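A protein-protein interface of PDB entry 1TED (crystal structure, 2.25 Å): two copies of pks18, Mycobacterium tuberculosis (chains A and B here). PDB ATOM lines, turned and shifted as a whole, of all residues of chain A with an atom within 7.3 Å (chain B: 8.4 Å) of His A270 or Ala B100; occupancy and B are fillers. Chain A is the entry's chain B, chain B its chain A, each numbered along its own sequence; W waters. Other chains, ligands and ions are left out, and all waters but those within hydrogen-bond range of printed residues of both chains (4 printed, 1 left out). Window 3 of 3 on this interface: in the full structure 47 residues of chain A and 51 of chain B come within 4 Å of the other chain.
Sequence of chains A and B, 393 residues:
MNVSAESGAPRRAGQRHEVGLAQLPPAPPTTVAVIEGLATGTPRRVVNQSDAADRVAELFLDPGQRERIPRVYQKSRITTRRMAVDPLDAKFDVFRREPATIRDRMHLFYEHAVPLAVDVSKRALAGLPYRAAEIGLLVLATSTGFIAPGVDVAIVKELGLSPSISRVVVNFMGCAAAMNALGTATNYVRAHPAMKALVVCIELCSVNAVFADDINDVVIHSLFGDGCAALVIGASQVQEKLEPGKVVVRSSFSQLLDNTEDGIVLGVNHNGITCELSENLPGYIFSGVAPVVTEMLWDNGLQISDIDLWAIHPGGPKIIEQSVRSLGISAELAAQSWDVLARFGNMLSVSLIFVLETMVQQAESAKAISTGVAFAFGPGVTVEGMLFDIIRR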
ATOM      1  N   ARG A  97      15.780  -5.349   5.238  1.00  0.00           N
ATOM      2  CA  ARG A  97      15.090  -6.440   4.578  1.00  0.00           C
ATOM      3  C   ARG A  97      13.821  -5.975   3.881  1.00  0.00           C
ATOM      4  O   ARG A  97      13.253  -6.698   3.066  1.00  0.00           O
ATOM      5  CB  ARG A  97      14.779  -7.532   5.604  1.00  0.00           C
ATOM      6  CG  ARG A  97      16.030  -8.124   6.246  1.00  0.00           C
ATOM      7  CD  ARG A  97      15.704  -8.906   7.507  1.00  0.00           C
ATOM      8  NE  ARG A  97      16.900  -9.490   8.105  1.00  0.00           N
ATOM      9  CZ  ARG A  97      16.938 -10.048   9.311  1.00  0.00           C
ATOM     10  NH1 ARG A  97      15.840 -10.095  10.058  1.00  0.00           N
ATOM     11  NH2 ARG A  97      18.075 -10.559   9.771  1.00  0.00           N
ATOM     12  N   GLU A  98      13.385  -4.759   4.189  1.00  0.00           N
ATOM     13  CA  GLU A  98      12.176  -4.223   3.576  1.00  0.00           C
ATOM     14  C   GLU A  98      12.397  -3.705   2.163  1.00  0.00           C
ATOM     15  O   GLU A  98      13.480  -3.237   1.815  1.00  0.00           O
ATOM     16  CB  GLU A  98      11.604  -3.076   4.409  1.00  0.00           C
ATOM     17  CG  GLU A  98      11.269  -3.414   5.845  1.00  0.00           C
ATOM     18  CD  GLU A  98      10.248  -2.457   6.433  1.00  0.00           C
ATOM     19  OE1 GLU A  98      10.456  -1.226   6.363  1.00  0.00           O
ATOM     20  OE2 GLU A  98       9.227  -2.941   6.968  1.00  0.00           O
ATOM     21  N   PRO A  99      11.362  -3.797   1.320  1.00  0.00           N
ATOM     22  CA  PRO A  99      11.444  -3.320  -0.057  1.00  0.00           C
ATOM     23  C   PRO A  99      10.871  -1.906  -0.081  1.00  0.00           C
ATOM     24  O   PRO A  99      10.347  -1.426   0.930  1.00  0.00           O
ATOM     25  CB  PRO A  99      10.548  -4.295  -0.802  1.00  0.00           C
ATOM     26  CG  PRO A  99       9.435  -4.472   0.165  1.00  0.00           C
ATOM     27  CD  PRO A  99      10.175  -4.655   1.495  1.00  0.00           C
ATOM     28  N   ALA A 100      10.974  -1.246  -1.230  1.00  0.00           N
ATOM     29  CA  ALA A 100      10.437   0.099  -1.387  1.00  0.00           C
ATOM     30  C   ALA A 100      10.829   1.014  -0.235  1.00  0.00           C
ATOM     31  O   ALA A 100       9.974   1.464   0.524  1.00  0.00           O
ATOM     32  CB  ALA A 100       8.916   0.030  -1.496  1.00  0.00           C
ATOM     33  N   THR A 101      12.120   1.298  -0.110  1.00  0.00           N
ATOM     34  CA  THR A 101      12.590   2.159   0.967  1.00  0.00           C
ATOM     35  C   THR A 101      13.575   3.229   0.513  1.00  0.00           C
ATOM     36  O   THR A 101      14.179   3.896   1.358  1.00  0.00           O
ATOM     37  CB  THR A 101      13.283   1.331   2.097  1.00  0.00           C
ATOM     38  OG1 THR A 101      14.334   0.528   1.537  1.00  0.00           O
ATOM     39  CG2 THR A 101      12.278   0.432   2.805  1.00  0.00           C
ATOM     40  N   ILE A 102      13.751   3.406  -0.799  1.00  0.00           N
ATOM     41  CA  ILE A 102      14.714   4.412  -1.272  1.00  0.00           C
ATOM     42  C   ILE A 102      14.429   5.789  -0.716  1.00  0.00           C
ATOM     43  O   ILE A 102      15.351   6.476  -0.273  1.00  0.00           O
ATOM     44  CB  ILE A 102      14.766   4.564  -2.826  1.00  0.00           C
ATOM     45  CG1 ILE A 102      13.564   3.884  -3.456  1.00  0.00           C
ATOM     46  CG2 ILE A 102      16.105   4.079  -3.366  1.00  0.00           C
ATOM     47  CD1 ILE A 102      12.287   4.547  -3.101  1.00  0.00           C
ATOM     48  N   ARG A 103      13.159   6.190  -0.740  1.00  0.00           N
ATOM     49  CA  ARG A 103      12.790   7.510  -0.245  1.00  0.00           C
ATOM     50  C   ARG A 103      13.272   7.690   1.186  1.00  0.00           C
ATOM     51  O   ARG A 103      13.925   8.674   1.505  1.00  0.00           O
ATOM     52  CB  ARG A 103      11.272   7.731  -0.327  1.00  0.00           C
ATOM     53  CG  ARG A 103      10.844   9.206  -0.163  1.00  0.00           C
ATOM     54  CD  ARG A 103      11.283  10.060  -1.358  1.00  0.00           C
ATOM     55  NE  ARG A 103      11.155  11.499  -1.101  1.00  0.00           N
ATOM     56  CZ  ARG A 103      10.015  12.189  -1.139  1.00  0.00           C
ATOM     57  NH1 ARG A 103       8.865  11.589  -1.431  1.00  0.00           N
ATOM     58  NH2 ARG A 103      10.027  13.491  -0.884  1.00  0.00           N
ATOM     59  N   ARG A 105      15.577   6.139   2.640  1.00  0.00           N
ATOM     60  CA  ARG A 105      17.027   6.101   2.584  1.00  0.00           C
ATOM     61  C   ARG A 105      17.600   7.423   2.075  1.00  0.00           C
ATOM     62  O   ARG A 105      18.686   7.833   2.489  1.00  0.00           O
ATOM     63  CB  ARG A 105      17.479   4.928   1.705  1.00  0.00           C
ATOM     64  CG  ARG A 105      17.231   3.553   2.332  1.00  0.00           C
ATOM     65  CD  ARG A 105      17.525   2.424   1.347  1.00  0.00           C
ATOM     66  NE  ARG A 105      17.315   1.092   1.927  1.00  0.00           N
ATOM     67  CZ  ARG A 105      18.261   0.356   2.508  1.00  0.00           C
ATOM     68  NH1 ARG A 105      19.511   0.806   2.597  1.00  0.00           N
ATOM     69  NH2 ARG A 105      17.958  -0.841   2.995  1.00  0.00           N
ATOM     70  N   VAL A 210      22.114  -3.092   1.527  1.00  0.00           N
ATOM     71  CA  VAL A 210      21.023  -4.043   1.367  1.00  0.00           C
ATOM     72  C   VAL A 210      21.434  -5.498   1.626  1.00  0.00           C
ATOM     73  O   VAL A 210      20.597  -6.338   1.980  1.00  0.00           O
ATOM     74  CB  VAL A 210      20.429  -3.928  -0.056  1.00  0.00           C
ATOM     75  CG1 VAL A 210      19.476  -5.071  -0.321  1.00  0.00           C
ATOM     76  CG2 VAL A 210      19.704  -2.603  -0.204  1.00  0.00           C
ATOM     77  N   VAL A 268      19.211   3.068  -9.621  1.00  0.00           N
ATOM     78  CA  VAL A 268      18.417   3.347  -8.440  1.00  0.00           C
ATOM     79  C   VAL A 268      17.385   2.232  -8.278  1.00  0.00           C
ATOM     80  O   VAL A 268      16.511   2.055  -9.133  1.00  0.00           O
ATOM     81  CB  VAL A 268      17.682   4.701  -8.560  1.00  0.00           C
ATOM     82  CG1 VAL A 268      16.762   4.889  -7.382  1.00  0.00           C
ATOM     83  CG2 VAL A 268      18.689   5.844  -8.625  1.00  0.00           C
ATOM     84  N   ASN A 269      17.508   1.464  -7.195  1.00  0.00           N
ATOM     85  CA  ASN A 269      16.565   0.383  -6.918  1.00  0.00           C
ATOM     86  C   ASN A 269      15.558   0.808  -5.842  1.00  0.00           C
ATOM     87  O   ASN A 269      15.805   1.744  -5.072  1.00  0.00           O
ATOM     88  CB  ASN A 269      17.297  -0.891  -6.466  1.00  0.00           C
ATOM     89  CG  ASN A 269      18.074  -1.559  -7.597  1.00  0.00           C
ATOM     90  OD1 ASN A 269      17.689  -1.472  -8.764  1.00  0.00           O
ATOM     91  ND2 ASN A 269      19.164  -2.247  -7.249  1.00  0.00           N
ATOM     92  N   HIS A 270      14.430   0.101  -5.791  1.00  0.00           N
ATOM     93  CA  HIS A 270      13.374   0.400  -4.826  1.00  0.00           C
ATOM     94  C   HIS A 270      13.876   0.424  -3.391  1.00  0.00           C
ATOM     95  O   HIS A 270      13.248   1.027  -2.522  1.00  0.00           O
ATOM     96  CB  HIS A 270      12.251  -0.632  -4.908  1.00  0.00           C
ATOM     97  CG  HIS A 270      12.666  -2.002  -4.468  1.00  0.00           C
ATOM     98  ND1 HIS A 270      13.214  -2.929  -5.330  1.00  0.00           N
ATOM     99  CD2 HIS A 270      12.640  -2.590  -3.249  1.00  0.00           C
ATOM    100  CE1 HIS A 270      13.506  -4.030  -4.662  1.00  0.00           C
ATOM    101  NE2 HIS A 270      13.168  -3.851  -3.397  1.00  0.00           N
ATOM    102  N   ASN A 271      14.999  -0.242  -3.146  1.00  0.00           N
ATOM    103  CA  ASN A 271      15.555  -0.306  -1.805  1.00  0.00           C
ATOM    104  C   ASN A 271      16.950   0.275  -1.712  1.00  0.00           C
ATOM    105  O   ASN A 271      17.711  -0.078  -0.808  1.00  0.00           O
ATOM    106  CB  ASN A 271      15.578  -1.754  -1.312  1.00  0.00           C
ATOM    107  CG  ASN A 271      16.432  -2.648  -2.180  1.00  0.00           C
ATOM    108  OD1 ASN A 271      16.867  -2.254  -3.272  1.00  0.00           O
ATOM    109  ND2 ASN A 271      16.669  -3.868  -1.709  1.00  0.00           N
ATOM    110  N   GLY A 272      17.292   1.154  -2.647  1.00  0.00           N
ATOM    111  CA  GLY A 272      18.601   1.766  -2.592  1.00  0.00           C
ATOM    112  C   GLY A 272      19.340   1.907  -3.899  1.00  0.00           C
ATOM    113  O   GLY A 272      19.013   1.279  -4.911  1.00  0.00           O
ATOM    114  N   ILE A 273      20.354   2.758  -3.856  1.00  0.00           N
ATOM    115  CA  ILE A 273      21.216   3.027  -4.991  1.00  0.00           C
ATOM    116  C   ILE A 273      22.233   1.873  -5.107  1.00  0.00           C
ATOM    117  O   ILE A 273      22.711   1.354  -4.096  1.00  0.00           O
ATOM    118  CB  ILE A 273      21.910   4.385  -4.770  1.00  0.00           C
ATOM    119  CG1 ILE A 273      20.838   5.486  -4.794  1.00  0.00           C
ATOM    120  CG2 ILE A 273      23.000   4.614  -5.806  1.00  0.00           C
ATOM    121  CD1 ILE A 273      21.290   6.815  -4.293  1.00  0.00           C
ATOM    122  N   PHE B  95       1.523  -2.081 -14.702  1.00  0.00           N
ATOM    123  CA  PHE B  95       2.863  -1.761 -14.221  1.00  0.00           C
ATOM    124  C   PHE B  95       2.804  -0.498 -13.366  1.00  0.00           C
ATOM    125  O   PHE B  95       3.562  -0.344 -12.407  1.00  0.00           O
ATOM    126  CB  PHE B  95       3.772  -1.521 -15.425  1.00  0.00           C
ATOM    127  CG  PHE B  95       5.121  -0.973 -15.078  1.00  0.00           C
ATOM    128  CD1 PHE B  95       6.104  -1.794 -14.529  1.00  0.00           C
ATOM    129  CD2 PHE B  95       5.427   0.358 -15.339  1.00  0.00           C
ATOM    130  CE1 PHE B  95       7.374  -1.294 -14.249  1.00  0.00           C
ATOM    131  CE2 PHE B  95       6.690   0.866 -15.064  1.00  0.00           C
ATOM    132  CZ  PHE B  95       7.668   0.038 -14.518  1.00  0.00           C
ATOM    133  N   ARG B  97       0.604   0.425 -11.294  1.00  0.00           N
ATOM    134  CA  ARG B  97       0.122   0.195  -9.942  1.00  0.00           C
ATOM    135  C   ARG B  97       1.007  -0.676  -9.062  1.00  0.00           C
ATOM    136  O   ARG B  97       0.696  -0.897  -7.893  1.00  0.00           O
ATOM    137  CB  ARG B  97      -1.290  -0.394  -9.994  1.00  0.00           C
ATOM    138  CG  ARG B  97      -2.352   0.601 -10.442  1.00  0.00           C
ATOM    139  CD  ARG B  97      -3.750   0.073 -10.172  1.00  0.00           C
ATOM    140  NE  ARG B  97      -4.242  -0.784 -11.246  1.00  0.00           N
ATOM    141  CZ  ARG B  97      -4.666  -0.334 -12.423  1.00  0.00           C
ATOM    142  NH1 ARG B  97      -4.657   0.971 -12.678  1.00  0.00           N
ATOM    143  NH2 ARG B  97      -5.104  -1.186 -13.344  1.00  0.00           N
ATOM    144  N   GLU B  98       2.113  -1.165  -9.605  1.00  0.00           N
ATOM    145  CA  GLU B  98       2.993  -2.009  -8.812  1.00  0.00           C
ATOM    146  C   GLU B  98       4.055  -1.225  -8.066  1.00  0.00           C
ATOM    147  O   GLU B  98       4.493  -0.171  -8.512  1.00  0.00           O
ATOM    148  CB  GLU B  98       3.683  -3.038  -9.695  1.00  0.00           C
ATOM    149  CG  GLU B  98       2.740  -3.951 -10.428  1.00  0.00           C
ATOM    150  CD  GLU B  98       3.437  -5.200 -10.909  1.00  0.00           C
ATOM    151  OE1 GLU B  98       4.469  -5.074 -11.612  1.00  0.00           O
ATOM    152  OE2 GLU B  98       2.952  -6.306 -10.576  1.00  0.00           O
ATOM    153  N   PRO B  99       4.479  -1.736  -6.906  1.00  0.00           N
ATOM    154  CA  PRO B  99       5.506  -1.074  -6.102  1.00  0.00           C
ATOM    155  C   PRO B  99       6.906  -1.503  -6.530  1.00  0.00           C
ATOM    156  O   PRO B  99       7.076  -2.482  -7.258  1.00  0.00           O
ATOM    157  CB  PRO B  99       5.184  -1.551  -4.692  1.00  0.00           C
ATOM    158  CG  PRO B  99       4.765  -2.965  -4.939  1.00  0.00           C
ATOM    159  CD  PRO B  99       3.841  -2.826  -6.140  1.00  0.00           C
ATOM    160  N   ALA B 100       7.905  -0.749  -6.092  1.00  0.00           N
ATOM    161  CA  ALA B 100       9.291  -1.084  -6.381  1.00  0.00           C
ATOM    162  C   ALA B 100       9.687  -1.114  -7.856  1.00  0.00           C
ATOM    163  O   ALA B 100      10.558  -1.887  -8.240  1.00  0.00           O
ATOM    164  CB  ALA B 100       9.620  -2.440  -5.730  1.00  0.00           C
ATOM    165  N   THR B 101       9.075  -0.264  -8.672  1.00  0.00           N
ATOM    166  CA  THR B 101       9.391  -0.229 -10.097  1.00  0.00           C
ATOM    167  C   THR B 101      10.351   0.897 -10.511  1.00  0.00           C
ATOM    168  O   THR B 101      10.576   1.120 -11.706  1.00  0.00           O
ATOM    169  CB  THR B 101       8.104  -0.076 -10.931  1.00  0.00           C
ATOM    170  OG1 THR B 101       7.360   1.055 -10.449  1.00  0.00           O
ATOM    171  CG2 THR B 101       7.252  -1.345 -10.846  1.00  0.00           C
ATOM    172  N   ILE B 102      10.911   1.603  -9.534  1.00  0.00           N
ATOM    173  CA  ILE B 102      11.815   2.709  -9.830  1.00  0.00           C
ATOM    174  C   ILE B 102      12.967   2.378 -10.796  1.00  0.00           C
ATOM    175  O   ILE B 102      13.250   3.155 -11.719  1.00  0.00           O
ATOM    176  CB  ILE B 102      12.400   3.305  -8.532  1.00  0.00           C
ATOM    177  CG1 ILE B 102      13.235   4.549  -8.854  1.00  0.00           C
ATOM    178  CG2 ILE B 102      13.234   2.275  -7.821  1.00  0.00           C
ATOM    179  CD1 ILE B 102      12.449   5.657  -9.540  1.00  0.00           C
ATOM    180  N   ARG B 103      13.627   1.235 -10.597  1.00  0.00           N
ATOM    181  CA  ARG B 103      14.744   0.846 -11.466  1.00  0.00           C
ATOM    182  C   ARG B 103      14.309   0.638 -12.919  1.00  0.00           C
ATOM    183  O   ARG B 103      15.016   1.027 -13.846  1.00  0.00           O
ATOM    184  CB  ARG B 103      15.419  -0.431 -10.948  1.00  0.00           C
ATOM    185  CG  ARG B 103      16.726  -0.780 -11.668  1.00  0.00           C
ATOM    186  CD  ARG B 103      17.817   0.268 -11.421  1.00  0.00           C
ATOM    187  NE  ARG B 103      19.009   0.044 -12.240  1.00  0.00           N
ATOM    188  CZ  ARG B 103      19.949  -0.870 -11.995  1.00  0.00           C
ATOM    189  NH1 ARG B 103      19.866  -1.673 -10.937  1.00  0.00           N
ATOM    190  NH2 ARG B 103      20.975  -0.988 -12.820  1.00  0.00           N
ATOM    191  N   ASP B 104      13.147   0.024 -13.120  1.00  0.00           N
ATOM    192  CA  ASP B 104      12.655  -0.207 -14.472  1.00  0.00           C
ATOM    193  C   ASP B 104      12.242   1.084 -15.149  1.00  0.00           C
ATOM    194  O   ASP B 104      12.344   1.206 -16.368  1.00  0.00           O
ATOM    195  CB  ASP B 104      11.473  -1.183 -14.464  1.00  0.00           C
ATOM    196  CG  ASP B 104      11.904  -2.618 -14.211  1.00  0.00           C
ATOM    197  OD1 ASP B 104      13.111  -2.920 -14.365  1.00  0.00           O
ATOM    198  OD2 ASP B 104      11.037  -3.452 -13.871  1.00  0.00           O
ATOM    199  N   ARG B 105      11.783   2.049 -14.357  1.00  0.00           N
ATOM    200  CA  ARG B 105      11.352   3.339 -14.885  1.00  0.00           C
ATOM    201  C   ARG B 105      12.544   4.186 -15.349  1.00  0.00           C
ATOM    202  O   ARG B 105      12.417   4.984 -16.284  1.00  0.00           O
ATOM    203  CB  ARG B 105      10.523   4.084 -13.829  1.00  0.00           C
ATOM    204  CG  ARG B 105       9.132   3.478 -13.558  1.00  0.00           C
ATOM    205  CD  ARG B 105       8.539   4.068 -12.278  1.00  0.00           C
ATOM    206  NE  ARG B 105       7.205   3.579 -11.939  1.00  0.00           N
ATOM    207  CZ  ARG B 105       6.067   4.131 -12.351  1.00  0.00           C
ATOM    208  NH1 ARG B 105       6.081   5.203 -13.134  1.00  0.00           N
ATOM    209  NH2 ARG B 105       4.908   3.628 -11.948  1.00  0.00           N
ATOM    210  N   VAL B 268      12.870  10.638  -4.596  1.00  0.00           N
ATOM    211  CA  VAL B 268      12.810   9.395  -5.339  1.00  0.00           C
ATOM    212  C   VAL B 268      11.967   8.375  -4.578  1.00  0.00           C
ATOM    213  O   VAL B 268      12.324   7.985  -3.468  1.00  0.00           O
ATOM    214  CB  VAL B 268      14.242   8.813  -5.556  1.00  0.00           C
ATOM    215  CG1 VAL B 268      14.157   7.481  -6.286  1.00  0.00           C
ATOM    216  CG2 VAL B 268      15.108   9.801  -6.343  1.00  0.00           C
ATOM    217  N   ASN B 269      10.841   7.959  -5.154  1.00  0.00           N
ATOM    218  CA  ASN B 269      10.005   6.952  -4.511  1.00  0.00           C
ATOM    219  C   ASN B 269      10.213   5.604  -5.193  1.00  0.00           C
ATOM    220  O   ASN B 269      10.686   5.532  -6.332  1.00  0.00           O
ATOM    221  CB  ASN B 269       8.519   7.304  -4.588  1.00  0.00           C
ATOM    222  CG  ASN B 269       8.143   8.476  -3.709  1.00  0.00           C
ATOM    223  OD1 ASN B 269       8.690   8.655  -2.618  1.00  0.00           O
ATOM    224  ND2 ASN B 269       7.186   9.276  -4.177  1.00  0.00           N
ATOM    225  N   HIS B 270       9.835   4.543  -4.486  1.00  0.00           N
ATOM    226  CA  HIS B 270       9.978   3.177  -4.982  1.00  0.00           C
ATOM    227  C   HIS B 270       9.300   2.967  -6.325  1.00  0.00           C
ATOM    228  O   HIS B 270       9.683   2.077  -7.081  1.00  0.00           O
ATOM    229  CB  HIS B 270       9.401   2.180  -3.976  1.00  0.00           C
ATOM    230  CG  HIS B 270       7.914   2.260  -3.825  1.00  0.00           C
ATOM    231  ND1 HIS B 270       7.298   3.130  -2.949  1.00  0.00           N
ATOM    232  CD2 HIS B 270       6.918   1.583  -4.445  1.00  0.00           C
ATOM    233  CE1 HIS B 270       5.987   2.983  -3.035  1.00  0.00           C
ATOM    234  NE2 HIS B 270       5.730   2.051  -3.936  1.00  0.00           N
ATOM    235  N   ASN B 271       8.288   3.780  -6.611  1.00  0.00           N
ATOM    236  CA  ASN B 271       7.565   3.670  -7.868  1.00  0.00           C
ATOM    237  C   ASN B 271       7.791   4.847  -8.804  1.00  0.00           C
ATOM    238  O   ASN B 271       7.034   5.053  -9.748  1.00  0.00           O
ATOM    239  CB  ASN B 271       6.066   3.493  -7.608  1.00  0.00           C
ATOM    240  CG  ASN B 271       5.480   4.586  -6.712  1.00  0.00           C
ATOM    241  OD1 ASN B 271       6.201   5.443  -6.174  1.00  0.00           O
ATOM    242  ND2 ASN B 271       4.155   4.550  -6.542  1.00  0.00           N
ATOM    243  N   GLY B 272       8.838   5.617  -8.547  1.00  0.00           N
ATOM    244  CA  GLY B 272       9.129   6.743  -9.409  1.00  0.00           C
ATOM    245  C   GLY B 272       9.551   8.023  -8.715  1.00  0.00           C
ATOM    246  O   GLY B 272       9.406   8.184  -7.499  1.00  0.00           O
HETATM  247  O   HOH W   1      21.251  -4.180  -9.178  1.00  0.00           O
HETATM  248  O   HOH W   2       5.747  10.929  -2.154  1.00  0.00           O
HETATM  249  O   HOH W   3      13.251  -1.009  -8.383  1.00  0.00           O
HETATM  250  O   HOH W   4      14.274  11.506  -2.400  1.00  0.00           O
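The backbone NH (N) of Arg B103 sits close to the backbone carbonyl oxygen (O) of Val A268, at 3.3 Å. OD1 of Asn A269 lies within hydrogen-bond range of NH1 of Arg B103 (3.1 Å). O of Val B268 sits close to N of Arg A103 (3.4 Å). OD1 of Asn B269 sits at hydrogen-bond distance from NH1 of Arg A103, at 3.2 Å.
The backbone NH (N) of Ala B100 sits close to the backbone carbonyl oxygen (O) of His B270 (3.5 Å). N of Thr B101 is in hydrogen-bond range of O of His B270, 2.9 Å away. The backbone NH of Ile B102 lies within hydrogen-bond range of the backbone carbonyl oxygen of His B270. The backbone NH (N) of Ala A100 lies close to the backbone carbonyl oxygen (O) of His A270, at 3.5 Å. The backbone NH (N) of Thr A101 sits at hydrogen-bond distance from the backbone carbonyl oxygen (O) of His A270. The backbone carbonyl oxygen (O) of His A270 sits at hydrogen-bond distance from the backbone NH (N) of Ile A102.
Among the printed residues, merely in contact across the chains: Ala A100 with His B270, Ile A102 with Val B268, Ile A102 with Asn B269, Ile A102 with His B270, Val A268 with Ile B102, Val A268 with Val B268, Asn A269 with Ile B102, His A270 with Ala B100 and His A270 with Ile B102.
Of chain B, only Ala B100 (3.3 Å) and Ile B102 (3.2 Å) come within 4 Å of His A270. Of the printed residues of chain B, Val A268 touches Ile B102 (3.5 Å), Arg B103 (3.2 Å) and Val B268 (3.8 Å). Printed residues of chain B within 4 Å of Ala A100: His B270. Ile A273 touches none of the printed residues of chain B. The nearest residue of chain B that does not touch His A270 is His B270 (4.1 Å). The nearest residue of chain A that does not touch Ala B100 is Ala A100 (4.8 Å).
Printed residues of chain B that touch a printed residue of chain A: Ala B100, Ile B102, Arg B103, Val B268, Asn B269 and His B270. Hydrophobic or aromatic side chains of chain B that line the printed part of chain A: Ala B100, Ile B102, Val B268 and His B270. Of the 15 printed residues of chain A, 6 touch a printed residue of chain B. Among the printed residues, 13 pairs touch across the chains. Among the printed residues, no Asp or Glu carboxylate lies within 4 Å of a Lys or Arg side-chain nitrogen of the other chain.
Ile A102 touches Val B268, and with the chains exchanged Val A268 touches Ile B102. Ile A102 touches Asn B269, and with the chains exchanged Asn A269 touches Ile B102. Ile A102 touches His B270, and with the chains exchanged His A270 touches Ile B102. Arg A103 touches Val B268, and with the chains exchanged Val A268 touches Arg B103.
Water W4 bridges the backbone NH (N) of Val B268 (2.7 Å) and the guanidinium group (NE) of Arg A103 (3.4 Å). Water W3 lies within hydrogen-bond range of the backbone carbonyl oxygen of Ala B100 (2.8 Å), the backbone NH of His A270 (3.1 Å) and the backbone NH of Arg B103 (3.2 Å). Water W2 lies within hydrogen-bond range of ND2 of Asn B269 (3.0 Å) and NH1 of Arg A103 (3.3 Å). Water W1 bridges the guanidinium group of Arg B103 (3.4 Å) and the side-chain amide nitrogen of Asn A269 (3.4 Å).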
